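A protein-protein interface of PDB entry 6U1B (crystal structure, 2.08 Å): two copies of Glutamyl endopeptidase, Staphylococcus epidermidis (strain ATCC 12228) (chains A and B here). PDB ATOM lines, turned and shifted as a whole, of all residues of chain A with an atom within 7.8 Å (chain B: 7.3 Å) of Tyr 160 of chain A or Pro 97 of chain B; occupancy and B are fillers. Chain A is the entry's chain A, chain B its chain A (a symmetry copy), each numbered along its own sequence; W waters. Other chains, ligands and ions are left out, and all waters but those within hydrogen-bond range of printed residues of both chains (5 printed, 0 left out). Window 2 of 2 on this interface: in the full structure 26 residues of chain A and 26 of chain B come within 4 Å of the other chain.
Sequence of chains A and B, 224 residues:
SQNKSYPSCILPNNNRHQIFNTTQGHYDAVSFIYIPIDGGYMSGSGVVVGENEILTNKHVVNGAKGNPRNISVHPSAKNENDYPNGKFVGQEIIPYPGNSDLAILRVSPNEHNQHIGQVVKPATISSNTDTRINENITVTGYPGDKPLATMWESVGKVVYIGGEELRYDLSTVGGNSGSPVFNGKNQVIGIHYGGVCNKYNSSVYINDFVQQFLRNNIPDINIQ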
ATOM      1  N   THR A 131      14.724  10.088  24.805  1.00  0.00           N
ATOM      2  CA  THR A 131      13.889   9.879  23.624  1.00  0.00           C
ATOM      3  C   THR A 131      13.709  11.178  22.845  1.00  0.00           C
ATOM      4  O   THR A 131      13.307  12.201  23.409  1.00  0.00           O
ATOM      5  CB  THR A 131      12.520   9.332  24.029  1.00  0.00           C
ATOM      6  OG1 THR A 131      12.685   8.201  24.897  1.00  0.00           O
ATOM      7  CG2 THR A 131      11.731   8.921  22.783  1.00  0.00           C
ATOM      8  N   ARG A 132      13.967  11.135  21.537  1.00  0.00           N
ATOM      9  CA  ARG A 132      13.984  12.357  20.745  1.00  0.00           C
ATOM     10  C   ARG A 132      13.437  12.129  19.353  1.00  0.00           C
ATOM     11  O   ARG A 132      13.375  11.005  18.855  1.00  0.00           O
ATOM     12  CB  ARG A 132      15.391  12.929  20.622  1.00  0.00           C
ATOM     13  CG  ARG A 132      15.855  13.448  21.916  1.00  0.00           C
ATOM     14  CD  ARG A 132      17.266  13.851  21.891  1.00  0.00           C
ATOM     15  NE  ARG A 132      17.580  14.283  23.232  1.00  0.00           N
ATOM     16  CZ  ARG A 132      18.745  14.767  23.614  1.00  0.00           C
ATOM     17  NH1 ARG A 132      19.737  14.888  22.736  1.00  0.00           N
ATOM     18  NH2 ARG A 132      18.895  15.124  24.882  1.00  0.00           N
ATOM     19  N   ILE A 133      13.054  13.248  18.733  1.00  0.00           N
ATOM     20  CA  ILE A 133      12.682  13.270  17.328  1.00  0.00           C
ATOM     21  C   ILE A 133      13.787  12.656  16.475  1.00  0.00           C
ATOM     22  O   ILE A 133      14.976  12.839  16.752  1.00  0.00           O
ATOM     23  CB  ILE A 133      12.391  14.726  16.924  1.00  0.00           C
ATOM     24  CG1 ILE A 133      11.318  15.313  17.847  1.00  0.00           C
ATOM     25  CG2 ILE A 133      12.008  14.823  15.464  1.00  0.00           C
ATOM     26  CD1 ILE A 133      11.597  16.727  18.242  1.00  0.00           C
ATOM     27  N   ASN A 134      13.381  11.931  15.425  1.00  0.00           N
ATOM     28  CA  ASN A 134      14.226  11.254  14.435  1.00  0.00           C
ATOM     29  C   ASN A 134      14.900   9.996  14.982  1.00  0.00           C
ATOM     30  O   ASN A 134      15.733   9.391  14.293  1.00  0.00           O
ATOM     31  CB  ASN A 134      15.269  12.205  13.832  1.00  0.00           C
ATOM     32  CG  ASN A 134      14.628  13.415  13.174  1.00  0.00           C
ATOM     33  OD1 ASN A 134      15.001  14.562  13.443  1.00  0.00           O
ATOM     34  ND2 ASN A 134      13.642  13.164  12.319  1.00  0.00           N
ATOM     35  N   LYS A 157      10.542   6.088  12.407  1.00  0.00           N
ATOM     36  CA  LYS A 157      11.181   7.131  13.207  1.00  0.00           C
ATOM     37  C   LYS A 157      10.158   7.997  13.943  1.00  0.00           C
ATOM     38  O   LYS A 157       9.044   8.218  13.459  1.00  0.00           O
ATOM     39  CB  LYS A 157      12.052   8.048  12.329  1.00  0.00           C
ATOM     40  CG  LYS A 157      13.328   7.419  11.785  1.00  0.00           C
ATOM     41  CD  LYS A 157      14.009   8.369  10.789  1.00  0.00           C
ATOM     42  CE  LYS A 157      15.313   7.782  10.239  1.00  0.00           C
ATOM     43  NZ  LYS A 157      16.354   7.620  11.304  1.00  0.00           N
ATOM     44  N   VAL A 158      10.574   8.514  15.107  1.00  0.00           N
ATOM     45  CA  VAL A 158       9.796   9.509  15.849  1.00  0.00           C
ATOM     46  C   VAL A 158       9.797  10.829  15.084  1.00  0.00           C
ATOM     47  O   VAL A 158      10.862  11.333  14.700  1.00  0.00           O
ATOM     48  CB  VAL A 158      10.386   9.703  17.257  1.00  0.00           C
ATOM     49  CG1 VAL A 158       9.592  10.750  18.047  1.00  0.00           C
ATOM     50  CG2 VAL A 158      10.454   8.380  18.022  1.00  0.00           C
ATOM     51  N   VAL A 159       8.610  11.404  14.861  1.00  0.00           N
ATOM     52  CA  VAL A 159       8.503  12.706  14.192  1.00  0.00           C
ATOM     53  C   VAL A 159       7.988  13.820  15.101  1.00  0.00           C
ATOM     54  O   VAL A 159       7.972  14.983  14.669  1.00  0.00           O
ATOM     55  CB  VAL A 159       7.631  12.640  12.917  1.00  0.00           C
ATOM     56  CG1 VAL A 159       8.190  11.625  11.911  1.00  0.00           C
ATOM     57  CG2 VAL A 159       6.163  12.354  13.251  1.00  0.00           C
ATOM     58  N   TYR A 160       7.593  13.522  16.336  1.00  0.00           N
ATOM     59  CA  TYR A 160       6.946  14.509  17.192  1.00  0.00           C
ATOM     60  C   TYR A 160       6.871  13.949  18.605  1.00  0.00           C
ATOM     61  O   TYR A 160       6.535  12.775  18.791  1.00  0.00           O
ATOM     62  CB  TYR A 160       5.534  14.851  16.658  1.00  0.00           C
ATOM     63  CG  TYR A 160       4.647  15.731  17.540  1.00  0.00           C
ATOM     64  CD1 TYR A 160       3.974  15.205  18.637  1.00  0.00           C
ATOM     65  CD2 TYR A 160       4.456  17.077  17.249  1.00  0.00           C
ATOM     66  CE1 TYR A 160       3.153  15.997  19.431  1.00  0.00           C
ATOM     67  CE2 TYR A 160       3.635  17.874  18.041  1.00  0.00           C
ATOM     68  CZ  TYR A 160       2.993  17.329  19.129  1.00  0.00           C
ATOM     69  OH  TYR A 160       2.175  18.110  19.922  1.00  0.00           O
ATOM     70  N   ILE A 161       7.198  14.786  19.590  1.00  0.00           N
ATOM     71  CA  ILE A 161       7.060  14.450  21.006  1.00  0.00           C
ATOM     72  C   ILE A 161       6.527  15.688  21.711  1.00  0.00           C
ATOM     73  O   ILE A 161       7.156  16.749  21.657  1.00  0.00           O
ATOM     74  CB  ILE A 161       8.389  14.030  21.657  1.00  0.00           C
ATOM     75  CG1 ILE A 161       8.958  12.750  21.049  1.00  0.00           C
ATOM     76  CG2 ILE A 161       8.232  13.855  23.154  1.00  0.00           C
ATOM     77  CD1 ILE A 161      10.285  12.349  21.716  1.00  0.00           C
ATOM     78  N   GLY A 162       5.398  15.554  22.395  1.00  0.00           N
ATOM     79  CA  GLY A 162       4.852  16.683  23.118  1.00  0.00           C
ATOM     80  C   GLY A 162       3.734  16.294  24.058  1.00  0.00           C
ATOM     81  O   GLY A 162       2.758  15.650  23.647  1.00  0.00           O
ATOM     82  N   GLY A 163       3.862  16.699  25.314  1.00  0.00           N
ATOM     83  CA  GLY A 163       2.893  16.304  26.316  1.00  0.00           C
ATOM     84  C   GLY A 163       2.883  14.796  26.463  1.00  0.00           C
ATOM     85  O   GLY A 163       3.923  14.162  26.669  1.00  0.00           O
ATOM     86  N   GLU A 164       1.695  14.206  26.343  1.00  0.00           N
ATOM     87  CA  GLU A 164       1.537  12.761  26.392  1.00  0.00           C
ATOM     88  C   GLU A 164       1.439  12.126  24.998  1.00  0.00           C
ATOM     89  O   GLU A 164       0.876  11.037  24.853  1.00  0.00           O
ATOM     90  CB  GLU A 164       0.320  12.414  27.254  1.00  0.00           C
ATOM     91  CG  GLU A 164       0.440  12.939  28.700  1.00  0.00           C
ATOM     92  CD  GLU A 164      -0.784  12.654  29.568  1.00  0.00           C
ATOM     93  OE1 GLU A 164      -1.827  12.185  29.037  1.00  0.00           O
ATOM     94  OE2 GLU A 164      -0.711  12.921  30.789  1.00  0.00           O
ATOM     95  N   GLU A 165       1.970  12.780  23.969  1.00  0.00           N
ATOM     96  CA  GLU A 165       1.839  12.300  22.600  1.00  0.00           C
ATOM     97  C   GLU A 165       3.208  12.144  21.954  1.00  0.00           C
ATOM     98  O   GLU A 165       4.048  13.041  22.052  1.00  0.00           O
ATOM     99  CB  GLU A 165       0.971  13.250  21.759  1.00  0.00           C
ATOM    100  CG  GLU A 165       0.856  12.862  20.276  1.00  0.00           C
ATOM    101  CD  GLU A 165      -0.529  12.336  19.875  1.00  0.00           C
ATOM    102  OE1 GLU A 165      -0.878  12.439  18.670  1.00  0.00           O
ATOM    103  OE2 GLU A 165      -1.255  11.796  20.744  1.00  0.00           O
ATOM    104  N   LEU A 166       3.426  11.003  21.305  1.00  0.00           N
ATOM    105  CA  LEU A 166       4.596  10.761  20.468  1.00  0.00           C
ATOM    106  C   LEU A 166       4.113  10.202  19.137  1.00  0.00           C
ATOM    107  O   LEU A 166       3.349   9.229  19.105  1.00  0.00           O
ATOM    108  CB  LEU A 166       5.597   9.804  21.160  1.00  0.00           C
ATOM    109  CG  LEU A 166       6.904   9.426  20.438  1.00  0.00           C
ATOM    110  CD1 LEU A 166       8.014   8.997  21.412  1.00  0.00           C
ATOM    111  CD2 LEU A 166       6.674   8.323  19.389  1.00  0.00           C
ATOM    112  N   ARG A 167       4.552  10.812  18.044  1.00  0.00           N
ATOM    113  CA  ARG A 167       4.113  10.458  16.703  1.00  0.00           C
ATOM    114  C   ARG A 167       5.281   9.909  15.902  1.00  0.00           C
ATOM    115  O   ARG A 167       6.439  10.246  16.170  1.00  0.00           O
ATOM    116  CB  ARG A 167       3.524  11.678  15.968  1.00  0.00           C
ATOM    117  CG  ARG A 167       2.298  12.264  16.642  1.00  0.00           C
ATOM    118  CD  ARG A 167       1.965  13.683  16.100  1.00  0.00           C
ATOM    119  NE  ARG A 167       0.936  14.316  16.929  1.00  0.00           N
ATOM    120  CZ  ARG A 167       0.539  15.582  16.825  1.00  0.00           C
ATOM    121  NH1 ARG A 167       1.056  16.377  15.894  1.00  0.00           N
ATOM    122  NH2 ARG A 167      -0.399  16.043  17.649  1.00  0.00           N
ATOM    123  N   TYR A 168       4.962   9.086  14.895  1.00  0.00           N
ATOM    124  CA  TYR A 168       5.980   8.422  14.087  1.00  0.00           C
ATOM    125  C   TYR A 168       5.489   8.275  12.650  1.00  0.00           C
ATOM    126  O   TYR A 168       4.299   8.423  12.352  1.00  0.00           O
ATOM    127  CB  TYR A 168       6.357   7.049  14.662  1.00  0.00           C
ATOM    128  CG  TYR A 168       5.271   6.374  15.494  1.00  0.00           C
ATOM    129  CD1 TYR A 168       4.130   5.834  14.899  1.00  0.00           C
ATOM    130  CD2 TYR A 168       5.405   6.262  16.874  1.00  0.00           C
ATOM    131  CE1 TYR A 168       3.152   5.212  15.666  1.00  0.00           C
ATOM    132  CE2 TYR A 168       4.446   5.644  17.650  1.00  0.00           C
ATOM    133  CZ  TYR A 168       3.315   5.124  17.046  1.00  0.00           C
ATOM    134  OH  TYR A 168       2.364   4.506  17.838  1.00  0.00           O
ATOM    135  N   ASP A 169       6.427   7.960  11.757  1.00  0.00           N
ATOM    136  CA  ASP A 169       6.148   7.879  10.330  1.00  0.00           C
ATOM    137  C   ASP A 169       5.872   6.460   9.857  1.00  0.00           C
ATOM    138  O   ASP A 169       5.768   6.237   8.647  1.00  0.00           O
ATOM    139  CB  ASP A 169       7.307   8.485   9.525  1.00  0.00           C
ATOM    140  CG  ASP A 169       8.635   7.736   9.720  1.00  0.00           C
ATOM    141  OD1 ASP A 169       8.652   6.645  10.332  1.00  0.00           O
ATOM    142  OD2 ASP A 169       9.672   8.237   9.242  1.00  0.00           O
ATOM    143  N   TYR A 200       0.662  10.703   9.907  1.00  0.00           N
ATOM    144  CA  TYR A 200       1.436  10.139  10.997  1.00  0.00           C
ATOM    145  C   TYR A 200       0.548   9.181  11.778  1.00  0.00           C
ATOM    146  O   TYR A 200      -0.677   9.200  11.647  1.00  0.00           O
ATOM    147  CB  TYR A 200       1.986  11.226  11.925  1.00  0.00           C
ATOM    148  CG  TYR A 200       0.964  12.086  12.662  1.00  0.00           C
ATOM    149  CD1 TYR A 200       0.279  11.605  13.787  1.00  0.00           C
ATOM    150  CD2 TYR A 200       0.716  13.403  12.267  1.00  0.00           C
ATOM    151  CE1 TYR A 200      -0.649  12.407  14.476  1.00  0.00           C
ATOM    152  CE2 TYR A 200      -0.206  14.207  12.953  1.00  0.00           C
ATOM    153  CZ  TYR A 200      -0.877  13.706  14.060  1.00  0.00           C
ATOM    154  OH  TYR A 200      -1.773  14.502  14.748  1.00  0.00           O
ATOM    155  N   ASN A 201       1.186   8.341  12.588  1.00  0.00           N
ATOM    156  CA  ASN A 201       0.503   7.543  13.592  1.00  0.00           C
ATOM    157  C   ASN A 201       0.978   7.996  14.967  1.00  0.00           C
ATOM    158  O   ASN A 201       2.021   8.645  15.098  1.00  0.00           O
ATOM    159  CB  ASN A 201       0.729   6.039  13.343  1.00  0.00           C
ATOM    160  CG  ASN A 201      -0.089   5.532  12.166  1.00  0.00           C
ATOM    161  OD1 ASN A 201      -1.270   5.868  12.041  1.00  0.00           O
ATOM    162  ND2 ASN A 201       0.536   4.764  11.274  1.00  0.00           N
ATOM    163  N   SER A 202       0.176   7.691  15.997  1.00  0.00           N
ATOM    164  CA  SER A 202       0.298   8.340  17.294  1.00  0.00           C
ATOM    165  C   SER A 202       0.320   7.321  18.422  1.00  0.00           C
ATOM    166  O   SER A 202      -0.351   6.288  18.360  1.00  0.00           O
ATOM    167  CB  SER A 202      -0.872   9.299  17.549  1.00  0.00           C
ATOM    168  OG  SER A 202      -1.185  10.004  16.376  1.00  0.00           O
ATOM    169  N   SER A 203       1.049   7.658  19.481  1.00  0.00           N
ATOM    170  CA  SER A 203       1.103   6.847  20.685  1.00  0.00           C
ATOM    171  C   SER A 203       1.004   7.747  21.899  1.00  0.00           C
ATOM    172  O   SER A 203       1.250   8.955  21.827  1.00  0.00           O
ATOM    173  CB  SER A 203       2.393   6.028  20.788  1.00  0.00           C
ATOM    174  OG  SER A 203       3.523   6.884  20.867  1.00  0.00           O
ATOM    175  N   TYR A 205       2.696   8.933  24.953  1.00  0.00           N
ATOM    176  CA  TYR A 205       4.087   9.052  25.376  1.00  0.00           C
ATOM    177  C   TYR A 205       4.190   8.821  26.876  1.00  0.00           C
ATOM    178  O   TYR A 205       3.449   9.431  27.651  1.00  0.00           O
ATOM    179  CB  TYR A 205       4.602  10.435  25.011  1.00  0.00           C
ATOM    180  CG  TYR A 205       6.060  10.666  25.281  1.00  0.00           C
ATOM    181  CD1 TYR A 205       7.027   9.792  24.790  1.00  0.00           C
ATOM    182  CD2 TYR A 205       6.478  11.792  25.987  1.00  0.00           C
ATOM    183  CE1 TYR A 205       8.377  10.028  25.012  1.00  0.00           C
ATOM    184  CE2 TYR A 205       7.822  12.037  26.214  1.00  0.00           C
ATOM    185  CZ  TYR A 205       8.767  11.154  25.725  1.00  0.00           C
ATOM    186  OH  TYR A 205      10.103  11.396  25.953  1.00  0.00           O
ATOM    187  N   LYS B  58     -10.570  13.438  14.713  1.00  0.00           N
ATOM    188  CA  LYS B  58      -9.505  12.861  13.890  1.00  0.00           C
ATOM    189  C   LYS B  58      -9.834  11.425  13.480  1.00  0.00           C
ATOM    190  O   LYS B  58      -9.658  11.041  12.315  1.00  0.00           O
ATOM    191  CB  LYS B  58      -8.166  12.886  14.641  1.00  0.00           C
ATOM    192  CG  LYS B  58      -7.427  14.222  14.646  1.00  0.00           C
ATOM    193  CD  LYS B  58      -6.375  14.217  15.747  1.00  0.00           C
ATOM    194  CE  LYS B  58      -5.535  15.472  15.739  1.00  0.00           C
ATOM    195  NZ  LYS B  58      -4.802  15.630  17.025  1.00  0.00           N
ATOM    196  N   ILE B  94      -8.212  19.222   8.169  1.00  0.00           N
ATOM    197  CA  ILE B  94      -7.268  20.039   8.927  1.00  0.00           C
ATOM    198  C   ILE B  94      -7.213  19.517  10.357  1.00  0.00           C
ATOM    199  O   ILE B  94      -8.036  19.912  11.197  1.00  0.00           O
ATOM    200  CB  ILE B  94      -7.663  21.524   8.891  1.00  0.00           C
ATOM    201  CG1 ILE B  94      -7.939  21.944   7.443  1.00  0.00           C
ATOM    202  CG2 ILE B  94      -6.562  22.385   9.519  1.00  0.00           C
ATOM    203  CD1 ILE B  94      -8.399  23.354   7.306  1.00  0.00           C
ATOM    204  N   PRO B  95      -6.278  18.637  10.680  1.00  0.00           N
ATOM    205  CA  PRO B  95      -6.251  18.073  12.032  1.00  0.00           C
ATOM    206  C   PRO B  95      -5.777  19.106  13.032  1.00  0.00           C
ATOM    207  O   PRO B  95      -4.985  19.992  12.711  1.00  0.00           O
ATOM    208  CB  PRO B  95      -5.260  16.908  11.913  1.00  0.00           C
ATOM    209  CG  PRO B  95      -4.340  17.321  10.800  1.00  0.00           C
ATOM    210  CD  PRO B  95      -5.177  18.128   9.833  1.00  0.00           C
ATOM    211  N   TYR B  96      -6.300  19.009  14.246  1.00  0.00           N
ATOM    212  CA  TYR B  96      -5.797  19.850  15.321  1.00  0.00           C
ATOM    213  C   TYR B  96      -4.347  19.465  15.601  1.00  0.00           C
ATOM    214  O   TYR B  96      -4.059  18.280  15.815  1.00  0.00           O
ATOM    215  CB  TYR B  96      -6.653  19.690  16.572  1.00  0.00           C
ATOM    216  CG  TYR B  96      -6.151  20.422  17.793  1.00  0.00           C
ATOM    217  CD1 TYR B  96      -5.824  21.776  17.740  1.00  0.00           C
ATOM    218  CD2 TYR B  96      -6.028  19.767  19.007  1.00  0.00           C
ATOM    219  CE1 TYR B  96      -5.368  22.452  18.870  1.00  0.00           C
ATOM    220  CE2 TYR B  96      -5.588  20.426  20.132  1.00  0.00           C
ATOM    221  CZ  TYR B  96      -5.261  21.772  20.061  1.00  0.00           C
ATOM    222  OH  TYR B  96      -4.825  22.426  21.190  1.00  0.00           O
ATOM    223  N   PRO B  97      -3.407  20.417  15.577  1.00  0.00           N
ATOM    224  CA  PRO B  97      -1.994  20.060  15.803  1.00  0.00           C
ATOM    225  C   PRO B  97      -1.722  19.557  17.207  1.00  0.00           C
ATOM    226  O   PRO B  97      -0.717  18.866  17.416  1.00  0.00           O
ATOM    227  CB  PRO B  97      -1.245  21.379  15.530  1.00  0.00           C
ATOM    228  CG  PRO B  97      -2.200  22.193  14.690  1.00  0.00           C
ATOM    229  CD  PRO B  97      -3.566  21.830  15.188  1.00  0.00           C
ATOM    230  N   GLY B  98      -2.574  19.879  18.173  1.00  0.00           N
ATOM    231  CA  GLY B  98      -2.399  19.356  19.508  1.00  0.00           C
ATOM    232  C   GLY B  98      -2.801  17.891  19.590  1.00  0.00           C
ATOM    233  O   GLY B  98      -3.032  17.204  18.594  1.00  0.00           O
ATOM    234  N   ASN B  99      -2.916  17.421  20.824  1.00  0.00           N
ATOM    235  CA  ASN B  99      -3.017  15.990  21.079  1.00  0.00           C
ATOM    236  C   ASN B  99      -4.449  15.490  21.214  1.00  0.00           C
ATOM    237  O   ASN B  99      -4.639  14.300  21.485  1.00  0.00           O
ATOM    238  CB  ASN B  99      -2.223  15.643  22.336  1.00  0.00           C
ATOM    239  CG  ASN B  99      -0.770  16.059  22.225  1.00  0.00           C
ATOM    240  OD1 ASN B  99      -0.242  16.210  21.116  1.00  0.00           O
ATOM    241  ND2 ASN B  99      -0.115  16.254  23.367  1.00  0.00           N
ATOM    242  N   SER B 100      -5.442  16.361  21.017  1.00  0.00           N
ATOM    243  CA  SER B 100      -6.858  16.015  21.118  1.00  0.00           C
ATOM    244  C   SER B 100      -7.375  15.390  19.829  1.00  0.00           C
ATOM    245  O   SER B 100      -6.903  15.704  18.736  1.00  0.00           O
ATOM    246  CB  SER B 100      -7.693  17.267  21.420  1.00  0.00           C
ATOM    247  OG  SER B 100      -7.706  17.511  22.803  1.00  0.00           O
ATOM    248  N   LEU B 102      -9.501  15.848  17.512  1.00  0.00           N
ATOM    249  CA  LEU B 102     -10.271  16.931  16.912  1.00  0.00           C
ATOM    250  C   LEU B 102      -9.738  17.267  15.528  1.00  0.00           C
ATOM    251  O   LEU B 102      -8.526  17.398  15.337  1.00  0.00           O
ATOM    252  CB  LEU B 102     -10.221  18.196  17.780  1.00  0.00           C
ATOM    253  CG  LEU B 102     -10.938  19.431  17.222  1.00  0.00           C
ATOM    254  CD1 LEU B 102     -12.458  19.283  17.363  1.00  0.00           C
ATOM    255  CD2 LEU B 102     -10.434  20.707  17.894  1.00  0.00           C
ATOM    256  N   GLU B 164      -7.569  19.604  27.703  1.00  0.00           N
ATOM    257  CA  GLU B 164      -8.452  19.544  26.548  1.00  0.00           C
ATOM    258  C   GLU B 164      -9.534  18.466  26.684  1.00  0.00           C
ATOM    259  O   GLU B 164     -10.058  17.985  25.674  1.00  0.00           O
ATOM    260  CB  GLU B 164      -7.613  19.341  25.282  1.00  0.00           C
ATOM    261  CG  GLU B 164      -6.590  20.472  25.052  1.00  0.00           C
ATOM    262  CD  GLU B 164      -5.704  20.268  23.824  1.00  0.00           C
ATOM    263  OE1 GLU B 164      -5.742  19.171  23.205  1.00  0.00           O
ATOM    264  OE2 GLU B 164      -4.944  21.206  23.489  1.00  0.00           O
ATOM    265  N   PHE B 213      -6.748  27.499  17.544  1.00  0.00           N
ATOM    266  CA  PHE B 213      -6.769  26.667  16.350  1.00  0.00           C
ATOM    267  C   PHE B 213      -8.001  26.973  15.510  1.00  0.00           C
ATOM    268  O   PHE B 213      -7.912  27.133  14.286  1.00  0.00           O
ATOM    269  CB  PHE B 213      -6.715  25.189  16.761  1.00  0.00           C
ATOM    270  CG  PHE B 213      -7.077  24.227  15.664  1.00  0.00           C
ATOM    271  CD1 PHE B 213      -6.303  24.126  14.518  1.00  0.00           C
ATOM    272  CD2 PHE B 213      -8.172  23.384  15.804  1.00  0.00           C
ATOM    273  CE1 PHE B 213      -6.631  23.229  13.515  1.00  0.00           C
ATOM    274  CE2 PHE B 213      -8.507  22.479  14.810  1.00  0.00           C
ATOM    275  CZ  PHE B 213      -7.738  22.396  13.660  1.00  0.00           C
ATOM    276  N   ASN B 217      -7.944  29.035  11.656  1.00  0.00           N
ATOM    277  CA  ASN B 217      -8.365  28.330  10.455  1.00  0.00           C
ATOM    278  C   ASN B 217      -9.746  28.713   9.949  1.00  0.00           C
ATOM    279  O   ASN B 217     -10.016  28.515   8.763  1.00  0.00           O
ATOM    280  CB  ASN B 217      -8.341  26.808  10.685  1.00  0.00           C
ATOM    281  CG  ASN B 217      -6.929  26.241  10.696  1.00  0.00           C
ATOM    282  OD1 ASN B 217      -6.362  25.951   9.645  1.00  0.00           O
ATOM    283  ND2 ASN B 217      -6.362  26.082  11.885  1.00  0.00           N
HETATM  284  O   HOH W   1       1.261  20.694  19.082  1.00  0.00           O
HETATM  285  O   HOH W   2      -2.825  13.585  16.918  1.00  0.00           O
HETATM  286  O   HOH W   3      -2.413  16.950  13.880  1.00  0.00           O
HETATM  287  O   HOH W   4      -1.119  15.643  26.134  1.00  0.00           O
HETATM  288  O   HOH W   5       1.721  19.071  15.173  1.00  0.00           O
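The backbone carbonyl oxygen of Arg 167 of chain A is in hydrogen-bond range of the backbone NH of Val 159 of chain A (2.8 Å).
The side-chain carboxylate (OE1) of Glu 165 of chain A lies within salt-bridge range of the guanidinium group (NE) of Arg 167 of chain A, 3.1 Å away.
The side-chain carboxylate (OE1) of Glu 165 of chain A sits close to the side-chain hydroxyl (OG) of Ser 202 of chain A.
The guanidinium group of Arg 167 of chain A sits close to the side-chain hydroxyl of Tyr 200 of chain A (3.5 Å).
NZ of Lys 58 of chain B is in hydrogen-bond range of O of Tyr 96 of chain B.
The backbone carbonyl oxygen (O) of Gly 98 of chain B lies within hydrogen-bond range of the side-chain amino group (NZ) of Lys 58 of chain B (2.8 Å).
Position printed for both chains: 164.
Of the 8 pairs that touch across the chains among the printed residues, none has its exchanged pair printed and touching as well.
Water W2 lies within hydrogen-bond range of OH of Tyr 200 of chain A (2.6 Å), NZ of Lys 58 of chain B (2.8 Å) and OE1 of Glu 165 of chain A (2.9 Å).
Water W3 lies within hydrogen-bond range of OH of Tyr 200 of chain A (2.7 Å) and O of Tyr 96 of chain B (2.9 Å).
Water W5 bridges the guanidinium group (NH1) of Arg 167 of chain A (2.9 Å) and the backbone carbonyl oxygen (O) of Pro 97 of chain B (3.3 Å).
Water W1 bridges OH of Tyr 160 of chain A (2.9 Å) and O of Pro 97 of chain B (3.2 Å).
Water W4 bridges ND2 of Asn 99 of chain B (3.0 Å) and N of Glu 164 of chain A (3.2 Å).
Tyr 160 of chain A touches two residues of chain B.
Ile 161 of chain A touches none of the printed residues of chain B.
Of the printed residues of chain B, Gly 162 of chain A touches Asn 99 (2.9 Å).
Printed residues of chain B within 4 Å of Arg 167 of chain A: Pro 97, Gly 98 and Asn 99.
Pro 95 of chain B touches none of the printed residues of chain A.
Of chain A, only Tyr 160 (3.9 Å) and Arg 167 (2.9 Å) come within 4 Å of Pro 97 of chain B.
Gly 98 of chain B touches just one residue of chain A: Arg 167.
Of the printed residues of chain A, Asn 99 of chain B touches Tyr 160 (3.3 Å), Gly 162 (2.9 Å), Glu 165 (3.3 Å) and Arg 167 (3.5 Å).
The nearest residue of chain A that does not touch Pro 97 of chain B is Tyr 200 of chain A (5.2 Å).
The side-chain hydroxyl (OH) of Tyr 160 of chain A is in hydrogen-bond range of the side-chain amide oxygen (OD1) of Asn 99 of chain B, 3.3 Å away.
ND2 of Asn 99 of chain B lies within hydrogen-bond range of O of Gly 162 of chain A (2.9 Å).
The guanidinium group of Arg 167 of chain A lies within hydrogen-bond range of the backbone carbonyl oxygen of Pro 97 of chain B (2.9 Å).
The backbone carbonyl oxygen of Gly 98 of chain B lies within hydrogen-bond range of the guanidinium group of Arg 167 of chain A.
OD1 of Asn 99 of chain B lies within hydrogen-bond range of NH2 of Arg 167 of chain A, at 3.5 Å.
Of the 22 printed residues of chain A, 5 touch a printed residue of chain B.
Printed residues of chain A that touch a printed residue of chain B: Tyr 160, Gly 162, Glu 165, Arg 167 and Tyr 200.
Hydrophobic or aromatic side chains of chain A that line the printed part of chain B: Tyr 160 and Tyr 200.
Along chain B the printed residues that touch a printed residue of chain A span positions 58 to 99.
Among the printed residues, no Asp or Glu carboxylate lies within 4 Å of a Lys or Arg side-chain nitrogen of the other chain.
Among the printed residues, pairs that only touch across the chains: Glu 165 of chain A with Asn 99 of chain B, Tyr 160 of chain A with Pro 97 of chain B and Tyr 200 of chain A with Lys 58 of chain B.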
